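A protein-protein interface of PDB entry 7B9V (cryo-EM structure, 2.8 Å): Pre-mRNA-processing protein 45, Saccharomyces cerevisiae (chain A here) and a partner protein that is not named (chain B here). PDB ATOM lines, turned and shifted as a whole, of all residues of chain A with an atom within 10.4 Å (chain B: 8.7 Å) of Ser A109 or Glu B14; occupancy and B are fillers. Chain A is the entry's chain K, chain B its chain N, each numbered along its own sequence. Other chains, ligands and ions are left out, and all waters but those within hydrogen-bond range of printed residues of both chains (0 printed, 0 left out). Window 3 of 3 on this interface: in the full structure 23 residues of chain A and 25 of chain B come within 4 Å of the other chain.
The side-chain amide oxygen of Asn A107 sits close to the backbone carbonyl oxygen of Ile B12, 3.2 Å away.
A ring nitrogen (NE2) of His A110 is in hydrogen-bond range of the backbone carbonyl oxygen (O) of Gly B18 (2.8 Å).
The backbone carbonyl oxygen of Glu B20 sits close to a ring nitrogen (ND1) of His A110 (3.5 Å).
The backbone carbonyl oxygen of His A111 sits at hydrogen-bond distance from the backbone NH of Ile B23.
N of Ile A112 is in hydrogen-bond range of O of Leu A104 (2.9 Å).
Among the printed residues, merely in contact across the chains: His A111 with Asn B22, His A110 with Ile B23, Ile A112 with Ile B23, His A110 with Leu B17, Ser A109 with Glu B14, Asn A107 with Glu B14 and Asn A107 with Cys B13.
Ser A109 touches just one residue of chain B: Glu B14.
Printed residues of chain B within 4 Å of Ile A112: Ile B23 (3.5 Å).
Asn B11 touches none of the printed residues of chain A.
Of the printed residues of chain A, Ile B12 touches Asn A107 (3.2 Å).
Cys B13 touches just one residue of chain A: Asn A107 (3.8 Å).
Printed residues of chain A within 4 Å of Glu B14: Asn A107 (3.7 Å) and Ser A109 (3.6 Å).
Of chain A, only His A110 comes within 4 Å of Gly B18.
Cys B71 touches none of the printed residues of chain A.
Printed residues of chain A that touch a printed residue of chain B: Asn A107, Ser A109, His A110, His A111 and Ile A112.
Hydrophobic or aromatic side chains of chain A within 4 Å of the printed part of chain B: His A110, His A111 and Ile A112.
Among the printed residues, 11 pairs touch across the chains.
Among the printed residues, no Asp or Glu carboxylate lies within 4 Å of a Lys or Arg side-chain nitrogen of the other chain.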
ATOM      1  N   LEU A 104      13.286   2.426  13.722  1.00  0.00           N
ATOM      2  CA  LEU A 104      13.929   1.277  14.349  1.00  0.00           C
ATOM      3  C   LEU A 104      13.664   1.307  15.846  1.00  0.00           C
ATOM      4  O   LEU A 104      13.418   2.368  16.428  1.00  0.00           O
ATOM      5  CB  LEU A 104      15.451   1.238  14.107  1.00  0.00           C
ATOM      6  CG  LEU A 104      16.053   1.147  12.697  1.00  0.00           C
ATOM      7  CD1 LEU A 104      17.563   1.366  12.724  1.00  0.00           C
ATOM      8  CD2 LEU A 104      15.730  -0.192  12.064  1.00  0.00           C
ATOM      9  N   LEU A 105      13.716   0.128  16.463  1.00  0.00           N
ATOM     10  CA  LEU A 105      13.647  -0.005  17.913  1.00  0.00           C
ATOM     11  C   LEU A 105      14.932  -0.673  18.381  1.00  0.00           C
ATOM     12  O   LEU A 105      15.241  -1.792  17.958  1.00  0.00           O
ATOM     13  CB  LEU A 105      12.427  -0.828  18.334  1.00  0.00           C
ATOM     14  CG  LEU A 105      11.048  -0.347  17.869  1.00  0.00           C
ATOM     15  CD1 LEU A 105       9.974  -1.338  18.292  1.00  0.00           C
ATOM     16  CD2 LEU A 105      10.733   1.040  18.409  1.00  0.00           C
ATOM     17  N   LEU A 106      15.669   0.007  19.252  1.00  0.00           N
ATOM     18  CA  LEU A 106      16.978  -0.438  19.711  1.00  0.00           C
ATOM     19  C   LEU A 106      16.938  -0.682  21.206  1.00  0.00           C
ATOM     20  O   LEU A 106      16.441   0.183  21.940  1.00  0.00           O
ATOM     21  CB  LEU A 106      18.053   0.606  19.410  1.00  0.00           C
ATOM     22  CG  LEU A 106      18.282   1.010  17.959  1.00  0.00           C
ATOM     23  CD1 LEU A 106      19.510   1.893  17.877  1.00  0.00           C
ATOM     24  CD2 LEU A 106      18.419  -0.209  17.074  1.00  0.00           C
ATOM     25  N   ASN A 107      17.430  -1.853  21.662  1.00  0.00           N
ATOM     26  CA  ASN A 107      17.352  -2.269  23.076  1.00  0.00           C
ATOM     27  C   ASN A 107      15.928  -2.313  23.661  1.00  0.00           C
ATOM     28  O   ASN A 107      15.773  -2.188  24.882  1.00  0.00           O
ATOM     29  CB  ASN A 107      18.302  -1.459  23.979  1.00  0.00           C
ATOM     30  CG  ASN A 107      19.762  -1.846  23.771  1.00  0.00           C
ATOM     31  OD1 ASN A 107      20.150  -2.257  22.686  1.00  0.00           O
ATOM     32  ND2 ASN A 107      20.561  -1.724  24.823  1.00  0.00           N
ATOM     33  N   ASN A 108      14.892  -2.398  22.795  1.00  0.00           N
ATOM     34  CA  ASN A 108      13.448  -2.480  23.075  1.00  0.00           C
ATOM     35  C   ASN A 108      12.821  -1.236  23.695  1.00  0.00           C
ATOM     36  O   ASN A 108      11.590  -1.156  23.781  1.00  0.00           O
ATOM     37  CB  ASN A 108      13.096  -3.681  23.972  1.00  0.00           C
ATOM     38  CG  ASN A 108      13.755  -4.968  23.526  1.00  0.00           C
ATOM     39  OD1 ASN A 108      13.551  -5.439  22.407  1.00  0.00           O
ATOM     40  ND2 ASN A 108      14.578  -5.532  24.398  1.00  0.00           N
ATOM     41  N   SER A 109      13.619  -0.268  24.126  1.00  0.00           N
ATOM     42  CA  SER A 109      13.125   0.910  24.818  1.00  0.00           C
ATOM     43  C   SER A 109      13.044   2.115  23.894  1.00  0.00           C
ATOM     44  O   SER A 109      12.099   2.902  23.998  1.00  0.00           O
ATOM     45  CB  SER A 109      14.021   1.249  26.013  1.00  0.00           C
ATOM     46  OG  SER A 109      13.603   2.464  26.615  1.00  0.00           O
ATOM     47  N   HIS A 110      14.003   2.272  22.990  1.00  0.00           N
ATOM     48  CA  HIS A 110      14.221   3.530  22.298  1.00  0.00           C
ATOM     49  C   HIS A 110      13.645   3.459  20.890  1.00  0.00           C
ATOM     50  O   HIS A 110      13.929   2.513  20.147  1.00  0.00           O
ATOM     51  CB  HIS A 110      15.708   3.859  22.236  1.00  0.00           C
ATOM     52  CG  HIS A 110      16.195   4.607  23.434  1.00  0.00           C
ATOM     53  ND1 HIS A 110      15.807   5.900  23.704  1.00  0.00           N
ATOM     54  CD2 HIS A 110      17.051   4.255  24.424  1.00  0.00           C
ATOM     55  CE1 HIS A 110      16.393   6.312  24.812  1.00  0.00           C
ATOM     56  NE2 HIS A 110      17.156   5.334  25.267  1.00  0.00           N
ATOM     57  N   HIS A 111      12.839   4.456  20.529  1.00  0.00           N
ATOM     58  CA  HIS A 111      12.353   4.615  19.165  1.00  0.00           C
ATOM     59  C   HIS A 111      13.288   5.558  18.417  1.00  0.00           C
ATOM     60  O   HIS A 111      13.546   6.680  18.869  1.00  0.00           O
ATOM     61  CB  HIS A 111      10.923   5.159  19.162  1.00  0.00           C
ATOM     62  CG  HIS A 111      10.405   5.515  17.802  1.00  0.00           C
ATOM     63  ND1 HIS A 111       9.900   4.571  16.935  1.00  0.00           N
ATOM     64  CD2 HIS A 111      10.314   6.703  17.160  1.00  0.00           C
ATOM     65  CE1 HIS A 111       9.509   5.163  15.821  1.00  0.00           C
ATOM     66  NE2 HIS A 111       9.754   6.456  15.928  1.00  0.00           N
ATOM     67  N   ILE A 112      13.793   5.098  17.279  1.00  0.00           N
ATOM     68  CA  ILE A 112      14.831   5.790  16.530  1.00  0.00           C
ATOM     69  C   ILE A 112      14.260   6.238  15.191  1.00  0.00           C
ATOM     70  O   ILE A 112      13.736   5.420  14.426  1.00  0.00           O
ATOM     71  CB  ILE A 112      16.060   4.882  16.333  1.00  0.00           C
ATOM     72  CG1 ILE A 112      16.589   4.353  17.674  1.00  0.00           C
ATOM     73  CG2 ILE A 112      17.134   5.600  15.587  1.00  0.00           C
ATOM     74  CD1 ILE A 112      16.894   5.430  18.699  1.00  0.00           C
ATOM     75  N   ASN B  11      23.986  -1.624  16.702  1.00  0.00           N
ATOM     76  CA  ASN B  11      24.085  -2.133  18.080  1.00  0.00           C
ATOM     77  C   ASN B  11      24.575  -1.027  19.023  1.00  0.00           C
ATOM     78  O   ASN B  11      25.777  -0.831  19.207  1.00  0.00           O
ATOM     79  CB  ASN B  11      25.015  -3.371  18.082  1.00  0.00           C
ATOM     80  CG  ASN B  11      25.128  -4.085  19.455  1.00  0.00           C
ATOM     81  OD1 ASN B  11      24.551  -3.694  20.468  1.00  0.00           O
ATOM     82  ND2 ASN B  11      25.885  -5.175  19.449  1.00  0.00           N
ATOM     83  N   ILE B  12      23.629  -0.284  19.607  1.00  0.00           N
ATOM     84  CA  ILE B  12      23.896   0.873  20.468  1.00  0.00           C
ATOM     85  C   ILE B  12      23.212   0.640  21.815  1.00  0.00           C
ATOM     86  O   ILE B  12      22.043   0.241  21.856  1.00  0.00           O
ATOM     87  CB  ILE B  12      23.424   2.191  19.818  1.00  0.00           C
ATOM     88  CG1 ILE B  12      23.995   2.317  18.408  1.00  0.00           C
ATOM     89  CG2 ILE B  12      23.818   3.405  20.651  1.00  0.00           C
ATOM     90  CD1 ILE B  12      23.427   3.416  17.599  1.00  0.00           C
ATOM     91  N   CYS B  13      23.942   0.873  22.910  1.00  0.00           N
ATOM     92  CA  CYS B  13      23.447   0.689  24.275  1.00  0.00           C
ATOM     93  C   CYS B  13      22.585   1.872  24.716  1.00  0.00           C
ATOM     94  O   CYS B  13      22.643   2.962  24.143  1.00  0.00           O
ATOM     95  CB  CYS B  13      24.590   0.478  25.269  1.00  0.00           C
ATOM     96  SG  CYS B  13      25.661   1.901  25.572  1.00  0.00           S
ATOM     97  N   GLU B  14      21.745   1.620  25.735  1.00  0.00           N
ATOM     98  CA  GLU B  14      20.841   2.642  26.281  1.00  0.00           C
ATOM     99  C   GLU B  14      21.593   3.816  26.906  1.00  0.00           C
ATOM    100  O   GLU B  14      21.139   4.967  26.792  1.00  0.00           O
ATOM    101  CB  GLU B  14      19.890   2.000  27.302  1.00  0.00           C
ATOM    102  CG  GLU B  14      18.989   2.964  28.095  1.00  0.00           C
ATOM    103  CD  GLU B  14      17.848   2.271  28.818  1.00  0.00           C
ATOM    104  OE1 GLU B  14      18.119   1.449  29.721  1.00  0.00           O
ATOM    105  OE2 GLU B  14      16.678   2.548  28.476  1.00  0.00           O
ATOM    106  N   GLN B  15      22.753   3.563  27.520  1.00  0.00           N
ATOM    107  CA  GLN B  15      23.539   4.624  28.151  1.00  0.00           C
ATOM    108  C   GLN B  15      24.082   5.618  27.123  1.00  0.00           C
ATOM    109  O   GLN B  15      24.199   6.812  27.423  1.00  0.00           O
ATOM    110  CB  GLN B  15      24.668   4.030  28.999  1.00  0.00           C
ATOM    111  CG  GLN B  15      24.205   3.242  30.232  1.00  0.00           C
ATOM    112  CD  GLN B  15      24.013   1.756  29.989  1.00  0.00           C
ATOM    113  OE1 GLN B  15      23.775   1.328  28.870  1.00  0.00           O
ATOM    114  NE2 GLN B  15      24.124   0.974  31.052  1.00  0.00           N
ATOM    115  N   CYS B  16      24.396   5.147  25.912  1.00  0.00           N
ATOM    116  CA  CYS B  16      24.672   6.040  24.783  1.00  0.00           C
ATOM    117  C   CYS B  16      23.433   6.799  24.323  1.00  0.00           C
ATOM    118  O   CYS B  16      23.513   8.001  24.037  1.00  0.00           O
ATOM    119  CB  CYS B  16      25.283   5.276  23.610  1.00  0.00           C
ATOM    120  SG  CYS B  16      27.039   4.858  23.872  1.00  0.00           S
ATOM    121  N   LEU B  17      22.291   6.121  24.218  1.00  0.00           N
ATOM    122  CA  LEU B  17      21.113   6.754  23.643  1.00  0.00           C
ATOM    123  C   LEU B  17      20.465   7.739  24.604  1.00  0.00           C
ATOM    124  O   LEU B  17      19.761   8.650  24.149  1.00  0.00           O
ATOM    125  CB  LEU B  17      20.095   5.692  23.218  1.00  0.00           C
ATOM    126  CG  LEU B  17      20.519   4.744  22.092  1.00  0.00           C
ATOM    127  CD1 LEU B  17      19.593   3.539  22.010  1.00  0.00           C
ATOM    128  CD2 LEU B  17      20.557   5.479  20.766  1.00  0.00           C
ATOM    129  N   GLY B  18      20.682   7.581  25.905  1.00  0.00           N
ATOM    130  CA  GLY B  18      20.078   8.482  26.864  1.00  0.00           C
ATOM    131  C   GLY B  18      18.663   8.094  27.253  1.00  0.00           C
ATOM    132  O   GLY B  18      18.272   6.928  27.211  1.00  0.00           O
ATOM    133  N   ASP B  19      17.900   9.101  27.668  1.00  0.00           N
ATOM    134  CA  ASP B  19      16.585   8.871  28.235  1.00  0.00           C
ATOM    135  C   ASP B  19      15.469   9.631  27.537  1.00  0.00           C
ATOM    136  O   ASP B  19      14.326   9.575  28.008  1.00  0.00           O
ATOM    137  CB  ASP B  19      16.592   9.229  29.727  1.00  0.00           C
ATOM    138  CG  ASP B  19      16.959  10.684  29.979  1.00  0.00           C
ATOM    139  OD1 ASP B  19      17.567  11.322  29.090  1.00  0.00           O
ATOM    140  OD2 ASP B  19      16.635  11.198  31.069  1.00  0.00           O
ATOM    141  N   GLU B  20      15.770  10.397  26.487  1.00  0.00           N
ATOM    142  CA  GLU B  20      14.715  11.039  25.717  1.00  0.00           C
ATOM    143  C   GLU B  20      13.890   9.989  24.988  1.00  0.00           C
ATOM    144  O   GLU B  20      14.396   8.918  24.639  1.00  0.00           O
ATOM    145  CB  GLU B  20      15.304  12.044  24.720  1.00  0.00           C
ATOM    146  CG  GLU B  20      16.090  13.205  25.344  1.00  0.00           C
ATOM    147  CD  GLU B  20      15.264  14.154  26.227  1.00  0.00           C
ATOM    148  OE1 GLU B  20      14.014  14.188  26.147  1.00  0.00           O
ATOM    149  OE2 GLU B  20      15.882  14.865  27.046  1.00  0.00           O
ATOM    150  N   ALA B  21      12.591  10.280  24.836  1.00  0.00           N
ATOM    151  CA  ALA B  21      11.670   9.315  24.243  1.00  0.00           C
ATOM    152  C   ALA B  21      12.005   9.034  22.782  1.00  0.00           C
ATOM    153  O   ALA B  21      11.849   7.902  22.312  1.00  0.00           O
ATOM    154  CB  ALA B  21      10.235   9.822  24.374  1.00  0.00           C
ATOM    155  N   ASN B  22      12.499  10.042  22.063  1.00  0.00           N
ATOM    156  CA  ASN B  22      12.801   9.917  20.647  1.00  0.00           C
ATOM    157  C   ASN B  22      14.192  10.453  20.349  1.00  0.00           C
ATOM    158  O   ASN B  22      14.593  11.497  20.874  1.00  0.00           O
ATOM    159  CB  ASN B  22      11.766  10.642  19.788  1.00  0.00           C
ATOM    160  CG  ASN B  22      10.384  10.051  19.933  1.00  0.00           C
ATOM    161  OD1 ASN B  22      10.147   8.904  19.556  1.00  0.00           O
ATOM    162  ND2 ASN B  22       9.461  10.828  20.486  1.00  0.00           N
ATOM    163  N   ILE B  23      14.922   9.727  19.508  1.00  0.00           N
ATOM    164  CA  ILE B  23      16.246  10.121  19.040  1.00  0.00           C
ATOM    165  C   ILE B  23      16.227  10.111  17.520  1.00  0.00           C
ATOM    166  O   ILE B  23      15.891   9.090  16.908  1.00  0.00           O
ATOM    167  CB  ILE B  23      17.376   9.232  19.600  1.00  0.00           C
ATOM    168  CG1 ILE B  23      17.571   9.461  21.103  1.00  0.00           C
ATOM    169  CG2 ILE B  23      18.680   9.422  18.852  1.00  0.00           C
ATOM    170  CD1 ILE B  23      16.847   8.553  21.993  1.00  0.00           C
ATOM    171  N   PHE B  46      24.202  10.499  15.991  1.00  0.00           N
ATOM    172  CA  PHE B  46      23.052  11.070  16.668  1.00  0.00           C
ATOM    173  C   PHE B  46      23.524  11.970  17.801  1.00  0.00           C
ATOM    174  O   PHE B  46      24.684  11.935  18.214  1.00  0.00           O
ATOM    175  CB  PHE B  46      22.146   9.949  17.219  1.00  0.00           C
ATOM    176  CG  PHE B  46      22.806   9.087  18.301  1.00  0.00           C
ATOM    177  CD1 PHE B  46      23.636   8.022  17.944  1.00  0.00           C
ATOM    178  CD2 PHE B  46      22.589   9.333  19.654  1.00  0.00           C
ATOM    179  CE1 PHE B  46      24.239   7.240  18.904  1.00  0.00           C
ATOM    180  CE2 PHE B  46      23.199   8.552  20.620  1.00  0.00           C
ATOM    181  CZ  PHE B  46      24.024   7.506  20.241  1.00  0.00           C
ATOM    182  N   THR B  48      22.046  13.106  21.841  1.00  0.00           N
ATOM    183  CA  THR B  48      21.108  12.675  22.882  1.00  0.00           C
ATOM    184  C   THR B  48      19.883  13.583  22.960  1.00  0.00           C
ATOM    185  O   THR B  48      18.786  13.122  23.292  1.00  0.00           O
ATOM    186  CB  THR B  48      21.812  12.622  24.240  1.00  0.00           C
ATOM    187  OG1 THR B  48      22.483  13.863  24.489  1.00  0.00           O
ATOM    188  CG2 THR B  48      22.829  11.488  24.271  1.00  0.00           C
ATOM    189  N   CYS B  71      29.025  -2.340  22.438  1.00  0.00           N
ATOM    190  CA  CYS B  71      28.377  -1.190  21.801  1.00  0.00           C
ATOM    191  C   CYS B  71      29.257  -0.554  20.718  1.00  0.00           C
ATOM    192  O   CYS B  71      30.458  -0.361  20.904  1.00  0.00           O
ATOM    193  CB  CYS B  71      28.047  -0.174  22.899  1.00  0.00           C
ATOM    194  SG  CYS B  71      27.415   1.436  22.422  1.00  0.00           S
ATOM    195  N   CYS B  74      30.653   3.153  22.206  1.00  0.00           N
ATOM    196  CA  CYS B  74      31.536   3.291  23.356  1.00  0.00           C
ATOM    197  C   CYS B  74      32.369   2.057  23.666  1.00  0.00           C
ATOM    198  O   CYS B  74      33.185   2.115  24.593  1.00  0.00           O
ATOM    199  CB  CYS B  74      30.722   3.665  24.604  1.00  0.00           C
ATOM    200  SG  CYS B  74      29.705   2.303  25.276  1.00  0.00           S
ATOM    201  N   SER B  78      27.983  -5.094  25.723  1.00  0.00           N
ATOM    202  CA  SER B  78      26.590  -4.731  25.490  1.00  0.00           C
ATOM    203  C   SER B  78      25.605  -5.374  26.467  1.00  0.00           C
ATOM    204  O   SER B  78      24.413  -5.060  26.400  1.00  0.00           O
ATOM    205  CB  SER B  78      26.211  -5.077  24.044  1.00  0.00           C
ATOM    206  OG  SER B  78      26.409  -6.450  23.748  1.00  0.00           O
ATOM    207  N   HIS B  81      28.236  -3.641  30.353  1.00  0.00           N
ATOM    208  CA  HIS B  81      28.673  -2.218  30.275  1.00  0.00           C
ATOM    209  C   HIS B  81      30.050  -2.000  30.928  1.00  0.00           C
ATOM    210  O   HIS B  81      30.268  -1.078  31.721  1.00  0.00           O
ATOM    211  CB  HIS B  81      27.572  -1.313  30.862  1.00  0.00           C
ATOM    212  CG  HIS B  81      27.741   0.161  30.606  1.00  0.00           C
ATOM    213  ND1 HIS B  81      27.533   0.736  29.362  1.00  0.00           N
ATOM    214  CD2 HIS B  81      28.033   1.183  31.451  1.00  0.00           C
ATOM    215  CE1 HIS B  81      27.719   2.035  29.454  1.00  0.00           C
ATOM    216  NE2 HIS B  81      28.025   2.334  30.711  1.00  0.00           N
